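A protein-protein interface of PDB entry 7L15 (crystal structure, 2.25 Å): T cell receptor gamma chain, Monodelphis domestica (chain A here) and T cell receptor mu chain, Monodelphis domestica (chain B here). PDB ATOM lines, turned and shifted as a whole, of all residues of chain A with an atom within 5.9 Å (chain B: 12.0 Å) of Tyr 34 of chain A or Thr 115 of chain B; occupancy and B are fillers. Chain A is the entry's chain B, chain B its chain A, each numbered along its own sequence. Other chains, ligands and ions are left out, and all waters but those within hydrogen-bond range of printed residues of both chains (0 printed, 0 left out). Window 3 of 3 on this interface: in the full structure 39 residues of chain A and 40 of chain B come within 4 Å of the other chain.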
ATOM      1  N   SER A  32      -7.639 -12.026 -13.848  1.00  0.00           N
ATOM      2  CA  SER A  32      -7.816 -10.752 -13.170  1.00  0.00           C
ATOM      3  C   SER A  32      -9.293 -10.399 -13.135  1.00  0.00           C
ATOM      4  O   SER A  32     -10.087 -10.863 -13.958  1.00  0.00           O
ATOM      5  CB  SER A  32      -7.024  -9.624 -13.860  1.00  0.00           C
ATOM      6  OG  SER A  32      -7.102  -8.423 -13.107  1.00  0.00           O
ATOM      7  N   ASP A  33      -9.647  -9.538 -12.186  1.00  0.00           N
ATOM      8  CA  ASP A  33     -11.021  -9.083 -12.054  1.00  0.00           C
ATOM      9  C   ASP A  33     -11.333  -7.855 -12.906  1.00  0.00           C
ATOM     10  O   ASP A  33     -12.513  -7.521 -13.084  1.00  0.00           O
ATOM     11  CB  ASP A  33     -11.329  -8.787 -10.588  1.00  0.00           C
ATOM     12  CG  ASP A  33     -12.801  -8.573 -10.341  1.00  0.00           C
ATOM     13  OD1 ASP A  33     -13.609  -9.367 -10.865  1.00  0.00           O
ATOM     14  OD2 ASP A  33     -13.149  -7.619  -9.622  1.00  0.00           O
ATOM     15  N   TYR A  34     -10.324  -7.177 -13.438  1.00  0.00           N
ATOM     16  CA  TYR A  34     -10.524  -5.911 -14.133  1.00  0.00           C
ATOM     17  C   TYR A  34     -10.305  -6.078 -15.631  1.00  0.00           C
ATOM     18  O   TYR A  34      -9.341  -6.724 -16.066  1.00  0.00           O
ATOM     19  CB  TYR A  34      -9.610  -4.830 -13.554  1.00  0.00           C
ATOM     20  CG  TYR A  34      -9.924  -4.601 -12.103  1.00  0.00           C
ATOM     21  CD1 TYR A  34     -10.905  -3.699 -11.720  1.00  0.00           C
ATOM     22  CD2 TYR A  34      -9.296  -5.347 -11.116  1.00  0.00           C
ATOM     23  CE1 TYR A  34     -11.224  -3.514 -10.382  1.00  0.00           C
ATOM     24  CE2 TYR A  34      -9.610  -5.174  -9.774  1.00  0.00           C
ATOM     25  CZ  TYR A  34     -10.570  -4.254  -9.414  1.00  0.00           C
ATOM     26  OH  TYR A  34     -10.877  -4.075  -8.090  1.00  0.00           O
ATOM     27  N   VAL A  35     -11.233  -5.528 -16.408  1.00  0.00           N
ATOM     28  CA  VAL A  35     -11.128  -5.443 -17.857  1.00  0.00           C
ATOM     29  C   VAL A  35     -10.906  -3.980 -18.203  1.00  0.00           C
ATOM     30  O   VAL A  35     -11.693  -3.117 -17.791  1.00  0.00           O
ATOM     31  CB  VAL A  35     -12.384  -5.996 -18.540  1.00  0.00           C
ATOM     32  CG1 VAL A  35     -12.258  -5.889 -20.051  1.00  0.00           C
ATOM     33  CG2 VAL A  35     -12.612  -7.446 -18.119  1.00  0.00           C
ATOM     34  N   HIS A  36      -9.829  -3.700 -18.941  1.00  0.00           N
ATOM     35  CA  HIS A  36      -9.417  -2.343 -19.282  1.00  0.00           C
ATOM     36  C   HIS A  36      -9.705  -2.066 -20.749  1.00  0.00           C
ATOM     37  O   HIS A  36      -9.550  -2.952 -21.588  1.00  0.00           O
ATOM     38  CB  HIS A  36      -7.926  -2.134 -19.007  1.00  0.00           C
ATOM     39  CG  HIS A  36      -7.504  -2.530 -17.628  1.00  0.00           C
ATOM     40  ND1 HIS A  36      -7.200  -1.604 -16.650  1.00  0.00           N
ATOM     41  CD2 HIS A  36      -7.330  -3.750 -17.061  1.00  0.00           C
ATOM     42  CE1 HIS A  36      -6.855  -2.236 -15.541  1.00  0.00           C
ATOM     43  NE2 HIS A  36      -6.925  -3.539 -15.764  1.00  0.00           N
ATOM     44  N   ARG A  48      -5.950   4.838 -21.877  1.00  0.00           N
ATOM     45  CA  ARG A  48      -7.045   4.079 -21.309  1.00  0.00           C
ATOM     46  C   ARG A  48      -8.253   4.988 -21.155  1.00  0.00           C
ATOM     47  O   ARG A  48      -8.120   6.160 -20.788  1.00  0.00           O
ATOM     48  CB  ARG A  48      -6.651   3.475 -19.965  1.00  0.00           C
ATOM     49  CG  ARG A  48      -7.677   2.444 -19.501  1.00  0.00           C
ATOM     50  CD  ARG A  48      -7.300   1.806 -18.173  1.00  0.00           C
ATOM     51  NE  ARG A  48      -7.524   2.724 -17.066  1.00  0.00           N
ATOM     52  CZ  ARG A  48      -7.278   2.437 -15.793  1.00  0.00           C
ATOM     53  NH1 ARG A  48      -6.792   1.248 -15.459  1.00  0.00           N
ATOM     54  NH2 ARG A  48      -7.512   3.348 -14.859  1.00  0.00           N
ATOM     55  N   VAL A  51     -11.921   1.455 -16.760  1.00  0.00           N
ATOM     56  CA  VAL A  51     -11.651   0.116 -16.259  1.00  0.00           C
ATOM     57  C   VAL A  51     -12.927  -0.427 -15.622  1.00  0.00           C
ATOM     58  O   VAL A  51     -13.690   0.311 -14.990  1.00  0.00           O
ATOM     59  CB  VAL A  51     -10.471   0.094 -15.265  1.00  0.00           C
ATOM     60  CG1 VAL A  51     -10.767   0.965 -14.049  1.00  0.00           C
ATOM     61  CG2 VAL A  51     -10.162  -1.336 -14.855  1.00  0.00           C
ATOM     62  N   TYR A  52     -13.172  -1.715 -15.821  1.00  0.00           N
ATOM     63  CA  TYR A  52     -14.401  -2.365 -15.403  1.00  0.00           C
ATOM     64  C   TYR A  52     -14.049  -3.534 -14.503  1.00  0.00           C
ATOM     65  O   TYR A  52     -13.207  -4.366 -14.863  1.00  0.00           O
ATOM     66  CB  TYR A  52     -15.201  -2.839 -16.618  1.00  0.00           C
ATOM     67  CG  TYR A  52     -16.400  -3.709 -16.299  1.00  0.00           C
ATOM     68  CD1 TYR A  52     -17.570  -3.161 -15.783  1.00  0.00           C
ATOM     69  CD2 TYR A  52     -16.370  -5.075 -16.544  1.00  0.00           C
ATOM     70  CE1 TYR A  52     -18.673  -3.960 -15.505  1.00  0.00           C
ATOM     71  CE2 TYR A  52     -17.466  -5.881 -16.272  1.00  0.00           C
ATOM     72  CZ  TYR A  52     -18.615  -5.322 -15.752  1.00  0.00           C
ATOM     73  OH  TYR A  52     -19.702  -6.129 -15.478  1.00  0.00           O
ATOM     74  N   SER A  53     -14.678  -3.577 -13.331  1.00  0.00           N
ATOM     75  CA  SER A  53     -14.543  -4.693 -12.402  1.00  0.00           C
ATOM     76  C   SER A  53     -15.649  -5.700 -12.703  1.00  0.00           C
ATOM     77  O   SER A  53     -16.833  -5.402 -12.517  1.00  0.00           O
ATOM     78  CB  SER A  53     -14.626  -4.201 -10.959  1.00  0.00           C
ATOM     79  OG  SER A  53     -14.558  -5.280 -10.043  1.00  0.00           O
ATOM     80  N   ARG A  54     -15.271  -6.893 -13.165  1.00  0.00           N
ATOM     81  CA  ARG A  54     -16.282  -7.883 -13.514  1.00  0.00           C
ATOM     82  C   ARG A  54     -17.100  -8.291 -12.287  1.00  0.00           C
ATOM     83  O   ARG A  54     -18.335  -8.350 -12.344  1.00  0.00           O
ATOM     84  CB  ARG A  54     -15.621  -9.100 -14.161  1.00  0.00           C
ATOM     85  CG  ARG A  54     -15.246  -8.902 -15.630  1.00  0.00           C
ATOM     86  CD  ARG A  54     -14.883 -10.229 -16.246  1.00  0.00           C
ATOM     87  NE  ARG A  54     -14.057 -10.988 -15.319  1.00  0.00           N
ATOM     88  CZ  ARG A  54     -13.809 -12.285 -15.431  1.00  0.00           C
ATOM     89  NH1 ARG A  54     -14.328 -12.974 -16.438  1.00  0.00           N
ATOM     90  NH2 ARG A  54     -13.046 -12.888 -14.531  1.00  0.00           N
ATOM     91  N   LYS A  56     -17.575  -6.739  -9.092  1.00  0.00           N
ATOM     92  CA  LYS A  56     -18.433  -5.638  -8.662  1.00  0.00           C
ATOM     93  C   LYS A  56     -19.301  -5.082  -9.796  1.00  0.00           C
ATOM     94  O   LYS A  56     -20.132  -4.206  -9.533  1.00  0.00           O
ATOM     95  CB  LYS A  56     -17.596  -4.504  -8.039  1.00  0.00           C
ATOM     96  CG  LYS A  56     -16.444  -4.999  -7.151  1.00  0.00           C
ATOM     97  CD  LYS A  56     -15.949  -3.951  -6.153  1.00  0.00           C
ATOM     98  CE  LYS A  56     -15.438  -2.674  -6.807  1.00  0.00           C
ATOM     99  NZ  LYS A  56     -14.163  -2.856  -7.576  1.00  0.00           N
ATOM    100  N   ALA A  98      -8.088  -4.952 -22.512  1.00  0.00           N
ATOM    101  CA  ALA A  98      -6.820  -5.415 -21.982  1.00  0.00           C
ATOM    102  C   ALA A  98      -7.038  -6.013 -20.603  1.00  0.00           C
ATOM    103  O   ALA A  98      -8.047  -5.744 -19.942  1.00  0.00           O
ATOM    104  CB  ALA A  98      -5.797  -4.285 -21.911  1.00  0.00           C
ATOM    105  N   SER A  99      -6.065  -6.818 -20.169  1.00  0.00           N
ATOM    106  CA  SER A  99      -6.094  -7.362 -18.817  1.00  0.00           C
ATOM    107  C   SER A  99      -4.682  -7.508 -18.270  1.00  0.00           C
ATOM    108  O   SER A  99      -3.777  -7.965 -18.974  1.00  0.00           O
ATOM    109  CB  SER A  99      -6.799  -8.724 -18.771  1.00  0.00           C
ATOM    110  OG  SER A  99      -6.967  -9.127 -17.428  1.00  0.00           O
ATOM    111  N   TRP A 100      -4.509  -7.131 -17.006  1.00  0.00           N
ATOM    112  CA  TRP A 100      -3.273  -7.415 -16.295  1.00  0.00           C
ATOM    113  C   TRP A 100      -3.107  -8.915 -16.105  1.00  0.00           C
ATOM    114  O   TRP A 100      -4.066  -9.623 -15.786  1.00  0.00           O
ATOM    115  CB  TRP A 100      -3.271  -6.732 -14.927  1.00  0.00           C
ATOM    116  CG  TRP A 100      -2.962  -5.269 -14.966  1.00  0.00           C
ATOM    117  CD1 TRP A 100      -3.802  -4.250 -14.636  1.00  0.00           C
ATOM    118  CD2 TRP A 100      -1.721  -4.659 -15.362  1.00  0.00           C
ATOM    119  NE1 TRP A 100      -3.163  -3.039 -14.802  1.00  0.00           N
ATOM    120  CE2 TRP A 100      -1.884  -3.265 -15.243  1.00  0.00           C
ATOM    121  CE3 TRP A 100      -0.491  -5.157 -15.809  1.00  0.00           C
ATOM    122  CZ2 TRP A 100      -0.871  -2.364 -15.552  1.00  0.00           C
ATOM    123  CZ3 TRP A 100       0.517  -4.261 -16.112  1.00  0.00           C
ATOM    124  CH2 TRP A 100       0.320  -2.878 -15.981  1.00  0.00           C
ATOM    125  N   ARG B 107       4.500   3.700 -18.830  1.00  0.00           N
ATOM    126  CA  ARG B 107       4.667   3.790 -17.386  1.00  0.00           C
ATOM    127  C   ARG B 107       3.425   3.238 -16.705  1.00  0.00           C
ATOM    128  O   ARG B 107       2.300   3.616 -17.051  1.00  0.00           O
ATOM    129  CB  ARG B 107       4.906   5.239 -16.920  1.00  0.00           C
ATOM    130  CG  ARG B 107       4.927   5.391 -15.370  1.00  0.00           C
ATOM    131  CD  ARG B 107       5.144   6.838 -14.890  1.00  0.00           C
ATOM    132  NE  ARG B 107       5.287   6.956 -13.432  1.00  0.00           N
ATOM    133  CZ  ARG B 107       4.636   7.840 -12.668  1.00  0.00           C
ATOM    134  NH1 ARG B 107       3.785   8.710 -13.206  1.00  0.00           N
ATOM    135  NH2 ARG B 107       4.852   7.875 -11.350  1.00  0.00           N
ATOM    136  N   ARG B 108       3.631   2.363 -15.727  1.00  0.00           N
ATOM    137  CA  ARG B 108       2.529   1.865 -14.922  1.00  0.00           C
ATOM    138  C   ARG B 108       2.199   2.888 -13.841  1.00  0.00           C
ATOM    139  O   ARG B 108       3.094   3.364 -13.139  1.00  0.00           O
ATOM    140  CB  ARG B 108       2.889   0.509 -14.310  1.00  0.00           C
ATOM    141  CG  ARG B 108       1.808  -0.042 -13.397  1.00  0.00           C
ATOM    142  CD  ARG B 108       2.102  -1.491 -13.019  1.00  0.00           C
ATOM    143  NE  ARG B 108       0.978  -2.030 -12.272  1.00  0.00           N
ATOM    144  CZ  ARG B 108       0.586  -3.296 -12.306  1.00  0.00           C
ATOM    145  NH1 ARG B 108       1.229  -4.179 -13.064  1.00  0.00           N
ATOM    146  NH2 ARG B 108      -0.466  -3.668 -11.595  1.00  0.00           N
ATOM    147  N   VAL B 109       0.919   3.249 -13.739  1.00  0.00           N
ATOM    148  CA  VAL B 109       0.441   4.322 -12.869  1.00  0.00           C
ATOM    149  C   VAL B 109      -0.830   3.853 -12.170  1.00  0.00           C
ATOM    150  O   VAL B 109      -1.726   3.301 -12.815  1.00  0.00           O
ATOM    151  CB  VAL B 109       0.170   5.612 -13.671  1.00  0.00           C
ATOM    152  CG1 VAL B 109      -0.604   6.619 -12.848  1.00  0.00           C
ATOM    153  CG2 VAL B 109       1.483   6.215 -14.175  1.00  0.00           C
ATOM    154  N   GLY B 110      -0.913   4.059 -10.861  1.00  0.00           N
ATOM    155  CA  GLY B 110      -2.148   3.793 -10.143  1.00  0.00           C
ATOM    156  C   GLY B 110      -1.870   3.399  -8.702  1.00  0.00           C
ATOM    157  O   GLY B 110      -0.795   3.653  -8.172  1.00  0.00           O
ATOM    158  N   ASN B 111      -2.873   2.757  -8.089  1.00  0.00           N
ATOM    159  CA  ASN B 111      -2.778   2.408  -6.673  1.00  0.00           C
ATOM    160  C   ASN B 111      -1.741   1.323  -6.425  1.00  0.00           C
ATOM    161  O   ASN B 111      -1.121   1.302  -5.358  1.00  0.00           O
ATOM    162  CB  ASN B 111      -4.140   1.966  -6.140  1.00  0.00           C
ATOM    163  CG  ASN B 111      -5.191   3.032  -6.309  1.00  0.00           C
ATOM    164  OD1 ASN B 111      -4.914   4.217  -6.117  1.00  0.00           O
ATOM    165  ND2 ASN B 111      -6.400   2.630  -6.690  1.00  0.00           N
ATOM    166  N   GLY B 112      -1.534   0.424  -7.386  1.00  0.00           N
ATOM    167  CA  GLY B 112      -0.589  -0.656  -7.192  1.00  0.00           C
ATOM    168  C   GLY B 112      -1.161  -1.996  -7.604  1.00  0.00           C
ATOM    169  O   GLY B 112      -0.424  -2.970  -7.777  1.00  0.00           O
ATOM    170  N   ASP B 113      -2.480  -2.054  -7.784  1.00  0.00           N
ATOM    171  CA  ASP B 113      -3.183  -3.297  -8.035  1.00  0.00           C
ATOM    172  C   ASP B 113      -3.628  -3.380  -9.493  1.00  0.00           C
ATOM    173  O   ASP B 113      -3.152  -2.623 -10.346  1.00  0.00           O
ATOM    174  CB  ASP B 113      -4.359  -3.398  -7.067  1.00  0.00           C
ATOM    175  CG  ASP B 113      -5.175  -2.126  -7.019  1.00  0.00           C
ATOM    176  OD1 ASP B 113      -5.066  -1.311  -7.956  1.00  0.00           O
ATOM    177  OD2 ASP B 113      -5.918  -1.937  -6.035  1.00  0.00           O
ATOM    178  N   ASP B 114      -4.560  -4.291  -9.770  1.00  0.00           N
ATOM    179  CA  ASP B 114      -5.043  -4.561 -11.114  1.00  0.00           C
ATOM    180  C   ASP B 114      -5.882  -3.432 -11.692  1.00  0.00           C
ATOM    181  O   ASP B 114      -6.355  -3.556 -12.831  1.00  0.00           O
ATOM    182  CB  ASP B 114      -5.851  -5.856 -11.122  1.00  0.00           C
ATOM    183  CG  ASP B 114      -4.978  -7.087 -11.283  1.00  0.00           C
ATOM    184  OD1 ASP B 114      -3.731  -6.985 -11.173  1.00  0.00           O
ATOM    185  OD2 ASP B 114      -5.551  -8.165 -11.542  1.00  0.00           O
ATOM    186  N   THR B 115      -6.089  -2.348 -10.951  1.00  0.00           N
ATOM    187  CA  THR B 115      -6.728  -1.169 -11.512  1.00  0.00           C
ATOM    188  C   THR B 115      -5.727  -0.197 -12.119  1.00  0.00           C
ATOM    189  O   THR B 115      -6.143   0.832 -12.659  1.00  0.00           O
ATOM    190  CB  THR B 115      -7.535  -0.438 -10.442  1.00  0.00           C
ATOM    191  OG1 THR B 115      -6.660  -0.095  -9.362  1.00  0.00           O
ATOM    192  CG2 THR B 115      -8.674  -1.319  -9.932  1.00  0.00           C
ATOM    193  N   ASP B 116      -4.429  -0.483 -12.008  1.00  0.00           N
ATOM    194  CA  ASP B 116      -3.404   0.385 -12.573  1.00  0.00           C
ATOM    195  C   ASP B 116      -3.578   0.506 -14.082  1.00  0.00           C
ATOM    196  O   ASP B 116      -4.086  -0.398 -14.752  1.00  0.00           O
ATOM    197  CB  ASP B 116      -1.998  -0.151 -12.250  1.00  0.00           C
ATOM    198  CG  ASP B 116      -1.599   0.073 -10.790  1.00  0.00           C
ATOM    199  OD1 ASP B 116      -2.420   0.625 -10.032  1.00  0.00           O
ATOM    200  OD2 ASP B 116      -0.466  -0.290 -10.402  1.00  0.00           O
ATOM    201  N   LYS B 117      -3.158   1.641 -14.618  1.00  0.00           N
ATOM    202  CA  LYS B 117      -3.131   1.839 -16.060  1.00  0.00           C
ATOM    203  C   LYS B 117      -1.698   1.974 -16.560  1.00  0.00           C
ATOM    204  O   LYS B 117      -0.756   2.236 -15.803  1.00  0.00           O
ATOM    205  CB  LYS B 117      -3.922   3.082 -16.479  1.00  0.00           C
ATOM    206  CG  LYS B 117      -3.409   4.351 -15.825  1.00  0.00           C
ATOM    207  CD  LYS B 117      -4.190   5.611 -16.234  1.00  0.00           C
ATOM    208  CE  LYS B 117      -3.498   6.850 -15.641  1.00  0.00           C
ATOM    209  NZ  LYS B 117      -3.971   8.159 -16.183  1.00  0.00           N
ATOM    210  N   LEU B 118      -1.563   1.781 -17.860  1.00  0.00           N
ATOM    211  CA  LEU B 118      -0.376   2.149 -18.602  1.00  0.00           C
ATOM    212  C   LEU B 118      -0.630   3.517 -19.215  1.00  0.00           C
ATOM    213  O   LEU B 118      -1.709   3.755 -19.763  1.00  0.00           O
ATOM    214  CB  LEU B 118      -0.085   1.109 -19.685  1.00  0.00           C
ATOM    215  CG  LEU B 118       0.303  -0.253 -19.105  1.00  0.00           C
ATOM    216  CD1 LEU B 118       0.514  -1.287 -20.210  1.00  0.00           C
ATOM    217  CD2 LEU B 118       1.575  -0.052 -18.296  1.00  0.00           C
ATOM    218  N   VAL B 119       0.325   4.431 -19.047  1.00  0.00           N
ATOM    219  CA  VAL B 119       0.372   5.674 -19.803  1.00  0.00           C
ATOM    220  C   VAL B 119       1.423   5.476 -20.877  1.00  0.00           C
ATOM    221  O   VAL B 119       2.518   4.976 -20.589  1.00  0.00           O
ATOM    222  CB  VAL B 119       0.698   6.894 -18.917  1.00  0.00           C
ATOM    223  CG1 VAL B 119       0.614   8.194 -19.740  1.00  0.00           C
ATOM    224  CG2 VAL B 119      -0.256   6.982 -17.769  1.00  0.00           C
ATOM    225  N   PHE B 120       1.079   5.821 -22.115  1.00  0.00           N
ATOM    226  CA  PHE B 120       1.941   5.611 -23.269  1.00  0.00           C
ATOM    227  C   PHE B 120       2.389   6.947 -23.852  1.00  0.00           C
ATOM    228  O   PHE B 120       1.680   7.950 -23.767  1.00  0.00           O
ATOM    229  CB  PHE B 120       1.226   4.816 -24.370  1.00  0.00           C
ATOM    230  CG  PHE B 120       0.914   3.377 -24.012  1.00  0.00           C
ATOM    231  CD1 PHE B 120       1.866   2.383 -24.185  1.00  0.00           C
ATOM    232  CD2 PHE B 120      -0.340   3.015 -23.562  1.00  0.00           C
ATOM    233  CE1 PHE B 120       1.582   1.070 -23.884  1.00  0.00           C
ATOM    234  CE2 PHE B 120      -0.634   1.686 -23.261  1.00  0.00           C
ATOM    235  CZ  PHE B 120       0.330   0.721 -23.420  1.00  0.00           C
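The backbone carbonyl oxygen of Asp 114 of chain B lies within hydrogen-bond range of a ring nitrogen (NE2) of His 36 of chain A, at 3.0 Å.
The backbone carbonyl oxygen of Thr 115 of chain B lies within hydrogen-bond range of the guanidinium group of Arg 48 of chain A (2.9 Å).
The backbone carbonyl oxygen of Asp 116 of chain B lies within hydrogen-bond range of the indole nitrogen of Trp 100 of chain A, at 2.8 Å.
The backbone carbonyl oxygen (O) of Asp 116 of chain B sits at hydrogen-bond distance from the guanidinium group (NH1) of Arg 48 of chain A (3.2 Å).
OD2 of Asp 114 of chain B sits close to OG of Ser 32 of chain A, at 2.2 Å.
Among the printed residues, merely in contact across the chains: Trp 100 of chain A with Arg 108 of chain B, Trp 100 of chain A with Asp 114 of chain B, Tyr 34 of chain A with Thr 115 of chain B, His 36 of chain A with Asp 116 of chain B, Tyr 34 of chain A with Asp 114 of chain B, Arg 48 of chain A with Lys 117 of chain B and Trp 100 of chain A with Leu 118 of chain B.
Tyr 34 of chain A touches just these residues of chain B: Asp 114 (3.5 Å) and Thr 115 (3.4 Å).
Thr 115 of chain B touches just these residues of chain A: Tyr 34 and Arg 48.
Of chain B, only Asp 114 comes within 4 Å of Ser 32 of chain A.
No residue of chain B comes within 4 Å of Asp 33 of chain A.
No residue of chain B comes within 4 Å of Val 35 of chain A.
His 36 of chain A touches two residues of chain B.
No residue of chain B comes within 4 Å of Val 51 of chain A.
No residue of chain B comes within 4 Å of Ser 53 of chain A.
No residue of chain B comes within 4 Å of Ala 98 of chain A.
No residue of chain B comes within 4 Å of Ser 99 of chain A.
Of the printed residues of chain B, Trp 100 of chain A touches Arg 108 (3.1 Å), Asp 114 (3.2 Å), Asp 116 (2.8 Å) and Leu 118 (3.9 Å).
Printed residues of chain B within 4 Å of Arg 48 of chain A: Thr 115, Asp 116 and Lys 117.
Of the printed residues of chain A, Asp 116 of chain B touches His 36, Arg 48 and Trp 100.
Of the printed residues of chain A, Lys 117 of chain B touches Arg 48 (3.5 Å).
The nearest residue of chain B that does not touch Tyr 34 of chain A is Asp 113 of chain B (5.8 Å).
The backbone NH (N) of Gly 112 of chain B lies within hydrogen-bond range of the side-chain carboxylate (OD1) of Asp 116 of chain B, 2.8 Å away.
The backbone carbonyl oxygen of Val 109 of chain B is in hydrogen-bond range of the backbone NH of Lys 117 of chain B (2.8 Å).
NH2 of Arg 108 of chain B lies within hydrogen-bond range of O of Asp 113 of chain B, at 3.1 Å.
The backbone NH of Ala 98 of chain A lies within hydrogen-bond range of the backbone carbonyl oxygen of His 36 of chain A, at 2.6 Å.
The side-chain carboxylate of Asp 116 of chain B sits at hydrogen-bond distance from the backbone NH of Asn 111 of chain B (2.9 Å).
The side-chain carboxylate of Asp 113 of chain B sits at hydrogen-bond distance from the side-chain hydroxyl of Thr 115 of chain B.
Of the 14 printed residues of chain B, 6 touch a printed residue of chain A.
Printed residues of chain B that touch a printed residue of chain A: Arg 108, Asp 114, Thr 115, Asp 116, Lys 117 and Leu 118.
Hydrophobic or aromatic side chains of chain B within 4 Å of the printed part of chain A: Leu 118.
Along chain B the printed residues that touch a printed residue of chain A span positions 108 to 118.
Hydrophobic or aromatic side chains of chain A that line the printed part of chain B: Tyr 34, His 36 and Trp 100.
Among the printed residues, no Asp or Glu carboxylate lies within 4 Å of a Lys or Arg side-chain nitrogen of the other chain.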
